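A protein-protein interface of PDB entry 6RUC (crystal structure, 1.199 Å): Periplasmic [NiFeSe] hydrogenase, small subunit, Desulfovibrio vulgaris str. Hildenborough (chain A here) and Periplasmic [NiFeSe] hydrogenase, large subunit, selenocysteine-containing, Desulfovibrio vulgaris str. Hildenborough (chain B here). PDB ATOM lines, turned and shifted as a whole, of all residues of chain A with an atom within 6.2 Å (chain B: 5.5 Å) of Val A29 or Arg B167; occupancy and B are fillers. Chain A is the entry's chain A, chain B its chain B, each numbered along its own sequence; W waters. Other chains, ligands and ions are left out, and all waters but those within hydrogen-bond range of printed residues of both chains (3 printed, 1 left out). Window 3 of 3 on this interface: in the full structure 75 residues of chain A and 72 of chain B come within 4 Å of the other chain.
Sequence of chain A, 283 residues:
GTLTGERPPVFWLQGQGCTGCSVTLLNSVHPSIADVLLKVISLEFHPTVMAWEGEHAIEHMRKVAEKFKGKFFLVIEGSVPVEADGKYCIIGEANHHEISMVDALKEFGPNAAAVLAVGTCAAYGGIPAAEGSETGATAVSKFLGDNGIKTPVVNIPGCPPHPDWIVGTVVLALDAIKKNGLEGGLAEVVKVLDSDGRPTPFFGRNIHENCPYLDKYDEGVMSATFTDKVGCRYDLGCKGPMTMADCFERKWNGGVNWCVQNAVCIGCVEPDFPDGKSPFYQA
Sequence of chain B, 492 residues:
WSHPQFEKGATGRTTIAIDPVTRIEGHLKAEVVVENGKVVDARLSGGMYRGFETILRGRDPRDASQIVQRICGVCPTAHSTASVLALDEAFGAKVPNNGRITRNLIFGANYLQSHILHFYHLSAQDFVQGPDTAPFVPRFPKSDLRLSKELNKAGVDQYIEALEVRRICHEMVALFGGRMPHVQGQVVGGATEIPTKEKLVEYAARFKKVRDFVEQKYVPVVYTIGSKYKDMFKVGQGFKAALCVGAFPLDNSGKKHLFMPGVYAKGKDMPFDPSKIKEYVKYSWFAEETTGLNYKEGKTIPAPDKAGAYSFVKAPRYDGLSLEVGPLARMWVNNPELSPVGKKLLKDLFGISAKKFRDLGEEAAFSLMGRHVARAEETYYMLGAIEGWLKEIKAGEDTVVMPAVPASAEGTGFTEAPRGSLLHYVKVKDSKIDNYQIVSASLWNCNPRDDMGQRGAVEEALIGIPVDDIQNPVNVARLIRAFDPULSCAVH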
ATOM      1  N   LEU A  26      18.604  -5.187 -33.266  1.00  0.00           N
ATOM      2  CA  LEU A  26      20.037  -5.226 -33.006  1.00  0.00           C
ATOM      3  C   LEU A  26      20.380  -6.076 -31.791  1.00  0.00           C
ATOM      4  O   LEU A  26      21.524  -6.519 -31.658  1.00  0.00           O
ATOM      5  CB  LEU A  26      20.601  -3.811 -32.802  1.00  0.00           C
ATOM      6  CG  LEU A  26      20.414  -2.808 -33.939  1.00  0.00           C
ATOM      7  CD1 LEU A  26      21.117  -1.516 -33.582  1.00  0.00           C
ATOM      8  CD2 LEU A  26      20.961  -3.350 -35.264  1.00  0.00           C
ATOM      9  N   ASN A  27      19.421  -6.310 -30.897  1.00  0.00           N
ATOM     10  CA  ASN A  27      19.669  -7.086 -29.686  1.00  0.00           C
ATOM     11  C   ASN A  27      19.465  -8.594 -29.872  1.00  0.00           C
ATOM     12  O   ASN A  27      19.552  -9.335 -28.895  1.00  0.00           O
ATOM     13  CB  ASN A  27      18.799  -6.587 -28.529  1.00  0.00           C
ATOM     14  CG  ASN A  27      19.237  -5.233 -27.999  1.00  0.00           C
ATOM     15  OD1 ASN A  27      20.396  -4.815 -28.127  1.00  0.00           O
ATOM     16  ND2 ASN A  27      18.295  -4.541 -27.383  1.00  0.00           N
ATOM     17  N   SER A  28      19.199  -9.070 -31.089  1.00  0.00           N
ATOM     18  CA  SER A  28      19.004 -10.505 -31.298  1.00  0.00           C
ATOM     19  C   SER A  28      20.222 -11.305 -30.826  1.00  0.00           C
ATOM     20  O   SER A  28      21.366 -10.975 -31.141  1.00  0.00           O
ATOM     21  CB  SER A  28      18.755 -10.763 -32.785  1.00  0.00           C
ATOM     22  OG  SER A  28      18.428 -12.119 -33.012  1.00  0.00           O
ATOM     23  N   VAL A  29      19.978 -12.383 -30.080  1.00  0.00           N
ATOM     24  CA  VAL A  29      21.085 -13.176 -29.539  1.00  0.00           C
ATOM     25  C   VAL A  29      21.483 -14.293 -30.483  1.00  0.00           C
ATOM     26  O   VAL A  29      22.662 -14.423 -30.848  1.00  0.00           O
ATOM     27  CB  VAL A  29      20.755 -13.742 -28.147  1.00  0.00           C
ATOM     28  CG1 VAL A  29      21.836 -14.718 -27.679  1.00  0.00           C
ATOM     29  CG2 VAL A  29      20.619 -12.621 -27.167  1.00  0.00           C
ATOM     30  N   HIS A  30      20.521 -15.116 -30.848  1.00  0.00           N
ATOM     31  CA  HIS A  30      20.748 -16.293 -31.667  1.00  0.00           C
ATOM     32  C   HIS A  30      19.637 -16.356 -32.702  1.00  0.00           C
ATOM     33  O   HIS A  30      18.488 -16.657 -32.350  1.00  0.00           O
ATOM     34  CB  HIS A  30      20.683 -17.566 -30.819  1.00  0.00           C
ATOM     35  CG  HIS A  30      21.828 -17.725 -29.866  1.00  0.00           C
ATOM     36  ND1 HIS A  30      21.649 -18.037 -28.535  1.00  0.00           N
ATOM     37  CD2 HIS A  30      23.166 -17.631 -30.054  1.00  0.00           C
ATOM     38  CE1 HIS A  30      22.827 -18.121 -27.942  1.00  0.00           C
ATOM     39  NE2 HIS A  30      23.764 -17.881 -28.841  1.00  0.00           N
ATOM     40  N   PRO A  31      19.920 -16.057 -33.980  1.00  0.00           N
ATOM     41  CA  PRO A  31      21.193 -15.583 -34.532  1.00  0.00           C
ATOM     42  C   PRO A  31      21.481 -14.134 -34.141  1.00  0.00           C
ATOM     43  O   PRO A  31      20.574 -13.343 -33.927  1.00  0.00           O
ATOM     44  CB  PRO A  31      20.970 -15.685 -36.045  1.00  0.00           C
ATOM     45  CG  PRO A  31      19.494 -15.476 -36.198  1.00  0.00           C
ATOM     46  CD  PRO A  31      18.871 -16.142 -35.005  1.00  0.00           C
ATOM     47  N   SER A  32      22.761 -13.800 -34.053  1.00  0.00           N
ATOM     48  CA  SER A  32      23.178 -12.431 -33.804  1.00  0.00           C
ATOM     49  C   SER A  32      22.801 -11.541 -34.984  1.00  0.00           C
ATOM     50  O   SER A  32      22.593 -12.009 -36.105  1.00  0.00           O
ATOM     51  CB  SER A  32      24.695 -12.386 -33.645  1.00  0.00           C
ATOM     52  OG  SER A  32      25.327 -12.700 -34.880  1.00  0.00           O
ATOM     53  N   ILE A  33      22.743 -10.229 -34.737  1.00  0.00           N
ATOM     54  CA  ILE A  33      22.397  -9.325 -35.830  1.00  0.00           C
ATOM     55  C   ILE A  33      23.428  -9.392 -36.962  1.00  0.00           C
ATOM     56  O   ILE A  33      23.065  -9.294 -38.140  1.00  0.00           O
ATOM     57  CB  ILE A  33      22.137  -7.886 -35.330  1.00  0.00           C
ATOM     58  CG1 ILE A  33      21.585  -7.016 -36.458  1.00  0.00           C
ATOM     59  CG2 ILE A  33      23.404  -7.236 -34.782  1.00  0.00           C
ATOM     60  CD1 ILE A  33      20.244  -7.470 -36.958  1.00  0.00           C
ATOM     61  N   PRO A 163      13.289  -9.137 -30.093  1.00  0.00           N
ATOM     62  CA  PRO A 163      13.984  -9.507 -31.337  1.00  0.00           C
ATOM     63  C   PRO A 163      13.598 -10.867 -31.861  1.00  0.00           C
ATOM     64  O   PRO A 163      13.533 -11.056 -33.082  1.00  0.00           O
ATOM     65  CB  PRO A 163      15.475  -9.430 -30.965  1.00  0.00           C
ATOM     66  CG  PRO A 163      15.514  -9.446 -29.482  1.00  0.00           C
ATOM     67  CD  PRO A 163      14.243  -8.757 -29.039  1.00  0.00           C
ATOM     68  N   ASP A 164      13.370 -11.834 -30.972  1.00  0.00           N
ATOM     69  CA  ASP A 164      13.027 -13.180 -31.416  1.00  0.00           C
ATOM     70  C   ASP A 164      11.707 -13.212 -32.178  1.00  0.00           C
ATOM     71  O   ASP A 164      11.508 -14.089 -33.026  1.00  0.00           O
ATOM     72  CB  ASP A 164      12.904 -14.158 -30.238  1.00  0.00           C
ATOM     73  CG  ASP A 164      14.195 -14.380 -29.472  1.00  0.00           C
ATOM     74  OD1 ASP A 164      15.286 -13.971 -29.928  1.00  0.00           O
ATOM     75  OD2 ASP A 164      14.100 -15.001 -28.374  1.00  0.00           O
ATOM     76  N   ASN A 253      16.151  -9.331 -23.248  1.00  0.00           N
ATOM     77  CA  ASN A 253      17.557  -8.924 -23.203  1.00  0.00           C
ATOM     78  C   ASN A 253      18.459 -10.040 -22.678  1.00  0.00           C
ATOM     79  O   ASN A 253      19.177  -9.894 -21.689  1.00  0.00           O
ATOM     80  CB  ASN A 253      17.720  -7.622 -22.407  1.00  0.00           C
ATOM     81  CG  ASN A 253      16.954  -6.483 -23.043  1.00  0.00           C
ATOM     82  OD1 ASN A 253      15.817  -6.174 -22.655  1.00  0.00           O
ATOM     83  ND2 ASN A 253      17.570  -5.850 -24.056  1.00  0.00           N
ATOM     84  N   GLY A 254      18.439 -11.160 -23.391  1.00  0.00           N
ATOM     85  CA  GLY A 254      19.268 -12.281 -22.999  1.00  0.00           C
ATOM     86  C   GLY A 254      18.756 -13.020 -21.793  1.00  0.00           C
ATOM     87  O   GLY A 254      19.538 -13.686 -21.095  1.00  0.00           O
ATOM     88  N   ALA B 162      31.518  -4.706 -31.763  1.00  0.00           N
ATOM     89  CA  ALA B 162      30.700  -3.703 -31.093  1.00  0.00           C
ATOM     90  C   ALA B 162      29.213  -4.049 -31.146  1.00  0.00           C
ATOM     91  O   ALA B 162      28.452  -3.611 -30.281  1.00  0.00           O
ATOM     92  CB  ALA B 162      30.957  -2.324 -31.715  1.00  0.00           C
ATOM     93  N   LEU B 163      28.764  -4.789 -32.171  1.00  0.00           N
ATOM     94  CA  LEU B 163      27.371  -5.236 -32.184  1.00  0.00           C
ATOM     95  C   LEU B 163      27.065  -6.082 -30.955  1.00  0.00           C
ATOM     96  O   LEU B 163      25.980  -5.975 -30.372  1.00  0.00           O
ATOM     97  CB  LEU B 163      27.073  -6.023 -33.460  1.00  0.00           C
ATOM     98  CG  LEU B 163      27.098  -5.248 -34.780  1.00  0.00           C
ATOM     99  CD1 LEU B 163      27.130  -6.202 -35.974  1.00  0.00           C
ATOM    100  CD2 LEU B 163      25.922  -4.277 -34.871  1.00  0.00           C
ATOM    101  N   GLU B 164      28.002  -6.947 -30.557  1.00  0.00           N
ATOM    102  CA  GLU B 164      27.810  -7.722 -29.337  1.00  0.00           C
ATOM    103  C   GLU B 164      27.971  -6.850 -28.095  1.00  0.00           C
ATOM    104  O   GLU B 164      27.193  -6.972 -27.139  1.00  0.00           O
ATOM    105  CB  GLU B 164      28.763  -8.917 -29.316  1.00  0.00           C
ATOM    106  CG  GLU B 164      28.629  -9.801 -28.082  1.00  0.00           C
ATOM    107  CD  GLU B 164      27.225 -10.383 -27.868  1.00  0.00           C
ATOM    108  OE1 GLU B 164      26.295 -10.113 -28.673  1.00  0.00           O
ATOM    109  OE2 GLU B 164      27.049 -11.127 -26.877  1.00  0.00           O
ATOM    110  N   VAL B 165      28.951  -5.940 -28.094  1.00  0.00           N
ATOM    111  CA  VAL B 165      29.169  -5.117 -26.909  1.00  0.00           C
ATOM    112  C   VAL B 165      27.951  -4.248 -26.613  1.00  0.00           C
ATOM    113  O   VAL B 165      27.537  -4.132 -25.454  1.00  0.00           O
ATOM    114  CB  VAL B 165      30.465  -4.303 -27.037  1.00  0.00           C
ATOM    115  CG1 VAL B 165      30.636  -3.351 -25.838  1.00  0.00           C
ATOM    116  CG2 VAL B 165      31.671  -5.233 -27.156  1.00  0.00           C
ATOM    117  N   ARG B 166      27.374  -3.603 -27.642  1.00  0.00           N
ATOM    118  CA  ARG B 166      26.214  -2.744 -27.393  1.00  0.00           C
ATOM    119  C   ARG B 166      25.019  -3.567 -26.925  1.00  0.00           C
ATOM    120  O   ARG B 166      24.221  -3.091 -26.115  1.00  0.00           O
ATOM    121  CB  ARG B 166      25.864  -1.863 -28.607  1.00  0.00           C
ATOM    122  CG  ARG B 166      25.408  -2.596 -29.885  1.00  0.00           C
ATOM    123  CD  ARG B 166      24.369  -1.823 -30.721  1.00  0.00           C
ATOM    124  NE  ARG B 166      23.202  -1.494 -29.902  1.00  0.00           N
ATOM    125  CZ  ARG B 166      22.337  -2.387 -29.433  1.00  0.00           C
ATOM    126  NH1 ARG B 166      22.417  -3.671 -29.770  1.00  0.00           N
ATOM    127  NH2 ARG B 166      21.352  -1.981 -28.636  1.00  0.00           N
ATOM    128  N   ARG B 167      24.893  -4.812 -27.404  1.00  0.00           N
ATOM    129  CA  ARG B 167      23.821  -5.686 -26.931  1.00  0.00           C
ATOM    130  C   ARG B 167      24.007  -6.006 -25.450  1.00  0.00           C
ATOM    131  O   ARG B 167      23.041  -5.990 -24.679  1.00  0.00           O
ATOM    132  CB  ARG B 167      23.785  -6.967 -27.775  1.00  0.00           C
ATOM    133  CG  ARG B 167      22.664  -7.925 -27.416  1.00  0.00           C
ATOM    134  CD  ARG B 167      22.780  -9.259 -28.133  1.00  0.00           C
ATOM    135  NE  ARG B 167      23.885 -10.032 -27.582  1.00  0.00           N
ATOM    136  CZ  ARG B 167      23.854 -10.573 -26.361  1.00  0.00           C
ATOM    137  NH1 ARG B 167      22.777 -10.447 -25.595  1.00  0.00           N
ATOM    138  NH2 ARG B 167      24.893 -11.237 -25.898  1.00  0.00           N
ATOM    139  N   ILE B 168      25.243  -6.297 -25.037  1.00  0.00           N
ATOM    140  CA  ILE B 168      25.558  -6.524 -23.625  1.00  0.00           C
ATOM    141  C   ILE B 168      25.214  -5.306 -22.774  1.00  0.00           C
ATOM    142  O   ILE B 168      24.720  -5.440 -21.648  1.00  0.00           O
ATOM    143  CB  ILE B 168      27.035  -6.945 -23.478  1.00  0.00           C
ATOM    144  CG1 ILE B 168      27.250  -8.332 -24.084  1.00  0.00           C
ATOM    145  CG2 ILE B 168      27.453  -6.907 -22.016  1.00  0.00           C
ATOM    146  CD1 ILE B 168      28.707  -8.683 -24.249  1.00  0.00           C
ATOM    147  N   CYS B 169      25.459  -4.100 -23.296  1.00  0.00           N
ATOM    148  CA  CYS B 169      25.059  -2.891 -22.575  1.00  0.00           C
ATOM    149  C   CYS B 169      23.557  -2.876 -22.316  1.00  0.00           C
ATOM    150  O   CYS B 169      23.106  -2.452 -21.241  1.00  0.00           O
ATOM    151  CB  CYS B 169      25.462  -1.647 -23.366  1.00  0.00           C
ATOM    152  SG  CYS B 169      27.233  -1.327 -23.466  1.00  0.00           S
ATOM    153  N   HIS B 170      22.762  -3.306 -23.293  1.00  0.00           N
ATOM    154  CA  HIS B 170      21.320  -3.381 -23.064  1.00  0.00           C
ATOM    155  C   HIS B 170      20.940  -4.466 -22.060  1.00  0.00           C
ATOM    156  O   HIS B 170      19.945  -4.302 -21.343  1.00  0.00           O
ATOM    157  CB  HIS B 170      20.546  -3.484 -24.373  1.00  0.00           C
ATOM    158  CG  HIS B 170      20.215  -2.140 -24.945  1.00  0.00           C
ATOM    159  ND1 HIS B 170      19.408  -1.972 -26.047  1.00  0.00           N
ATOM    160  CD2 HIS B 170      20.586  -0.893 -24.559  1.00  0.00           C
ATOM    161  CE1 HIS B 170      19.280  -0.684 -26.304  1.00  0.00           C
ATOM    162  NE2 HIS B 170      19.987  -0.009 -25.416  1.00  0.00           N
ATOM    163  N   GLU B 171      21.697  -5.568 -21.978  1.00  0.00           N
ATOM    164  CA  GLU B 171      21.491  -6.504 -20.874  1.00  0.00           C
ATOM    165  C   GLU B 171      21.726  -5.818 -19.536  1.00  0.00           C
ATOM    166  O   GLU B 171      20.980  -6.037 -18.576  1.00  0.00           O
ATOM    167  CB  GLU B 171      22.382  -7.742 -20.999  1.00  0.00           C
ATOM    168  CG  GLU B 171      22.093  -8.575 -22.241  1.00  0.00           C
ATOM    169  CD  GLU B 171      22.833  -9.916 -22.252  1.00  0.00           C
ATOM    170  OE1 GLU B 171      23.790 -10.095 -21.472  1.00  0.00           O
ATOM    171  OE2 GLU B 171      22.473 -10.791 -23.068  1.00  0.00           O
ATOM    172  N   MET B 172      22.757  -4.975 -19.457  1.00  0.00           N
ATOM    173  CA  MET B 172      23.002  -4.223 -18.230  1.00  0.00           C
ATOM    174  C   MET B 172      21.817  -3.332 -17.887  1.00  0.00           C
ATOM    175  O   MET B 172      21.407  -3.272 -16.726  1.00  0.00           O
ATOM    176  CB  MET B 172      24.288  -3.406 -18.342  1.00  0.00           C
ATOM    177  CG  MET B 172      25.562  -4.255 -18.356  1.00  0.00           C
ATOM    178  SD  MET B 172      27.009  -3.397 -18.996  1.00  0.00           S
ATOM    179  CE  MET B 172      27.096  -2.013 -17.849  1.00  0.00           C
HETATM  180  O   HOH W   1      23.896  -4.966 -31.813  1.00  0.00           O
HETATM  181  O   HOH W   2      22.346 -12.975 -20.913  1.00  0.00           O
HETATM  182  O   HOH W   3      20.163  -6.877 -24.936  1.00  0.00           O
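Val A29 touches just one residue of chain B: Arg B167.
Arg B167 touches just these residues of chain A: Asn A27 (3.3 Å), Ser A28 (3.7 Å) and Val A29 (3.4 Å).
Printed residues of chain B within 4 Å of Gly A254: Glu B171.
Printed residues of chain A within 4 Å of Glu B171: Asn A253 and Gly A254.
Printed residues of chain A within 4 Å of Arg B166: Leu A26 (3.5 Å) and Asn A27 (2.8 Å).
Printed residues of chain A within 4 Å of Leu B163: Ile A33 (3.9 Å).
The nearest printed residue of chain B that does not touch Val A29 is Glu B171 (4.9 Å).
The nearest printed residue of chain A that does not touch Arg B166 is Ile A33 (6.2 Å).
Of the 12 printed residues of chain A, 7 touch a printed residue of chain B.
Printed residues of chain A that touch a printed residue of chain B: Leu A26, Asn A27, Ser A28, Val A29, Ile A33, Asn A253 and Gly A254.
Hydrophobic or aromatic side chains of chain A within 4 Å of the printed part of chain B: Leu A26, Val A29 and Ile A33.
Of the 11 printed residues of chain B, 5 touch a printed residue of chain A.
Hydrophobic or aromatic side chains of chain B that line the printed part of chain A: Leu B163 and His B170.
OD1 of Asn A27 sits at hydrogen-bond distance from NH1 of Arg B166, at 2.8 Å.
ND1 of His B170 lies within hydrogen-bond range of ND2 of Asn A27, 3.1 Å away.
O of Leu A26 touches NH1 of Arg B166, at 3.5 Å.
Asn A27 touches Arg B167.
O of Ser A28 touches CD of Arg B167, 3.7 Å away.
NH1 of Arg B167 touches CG2 of Val A29 (3.4 Å).
Ile A33 touches Leu B163 (CG2 to CD2, 3.9 Å).
Asn A253 touches His B170.
O of Asn A253 touches CG of Glu B171 (3.2 Å).
OE2 of Glu B171 touches CA of Gly A254 (3.5 Å).
OG of Ser A28 is in hydrogen-bond range of O of Pro A31 (2.6 Å).
The side-chain carboxylate (OE1) of Glu B164 lies within salt-bridge range of the guanidinium group (NE) of Arg B167, at 2.6 Å.
The guanidinium group of Arg B166 is in hydrogen-bond range of a ring nitrogen (ND1) of His B170, at 3.2 Å.
The guanidinium group of Arg B167 is in salt-bridge range of the side-chain carboxylate of Glu B171, 2.6 Å away.
Water W1 lies within hydrogen-bond range of O of Leu B163 (2.7 Å), NH1 of Arg B166 (2.8 Å) and O of Leu A26 (2.8 Å).
Water W2 bridges the backbone carbonyl oxygen of Gly A254 and the side-chain carboxylate of Glu B171.
Water W3 lies within hydrogen-bond range of the side-chain amide nitrogen of Asn A253 (2.9 Å) and the backbone carbonyl oxygen of Arg B167 (3.0 Å).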
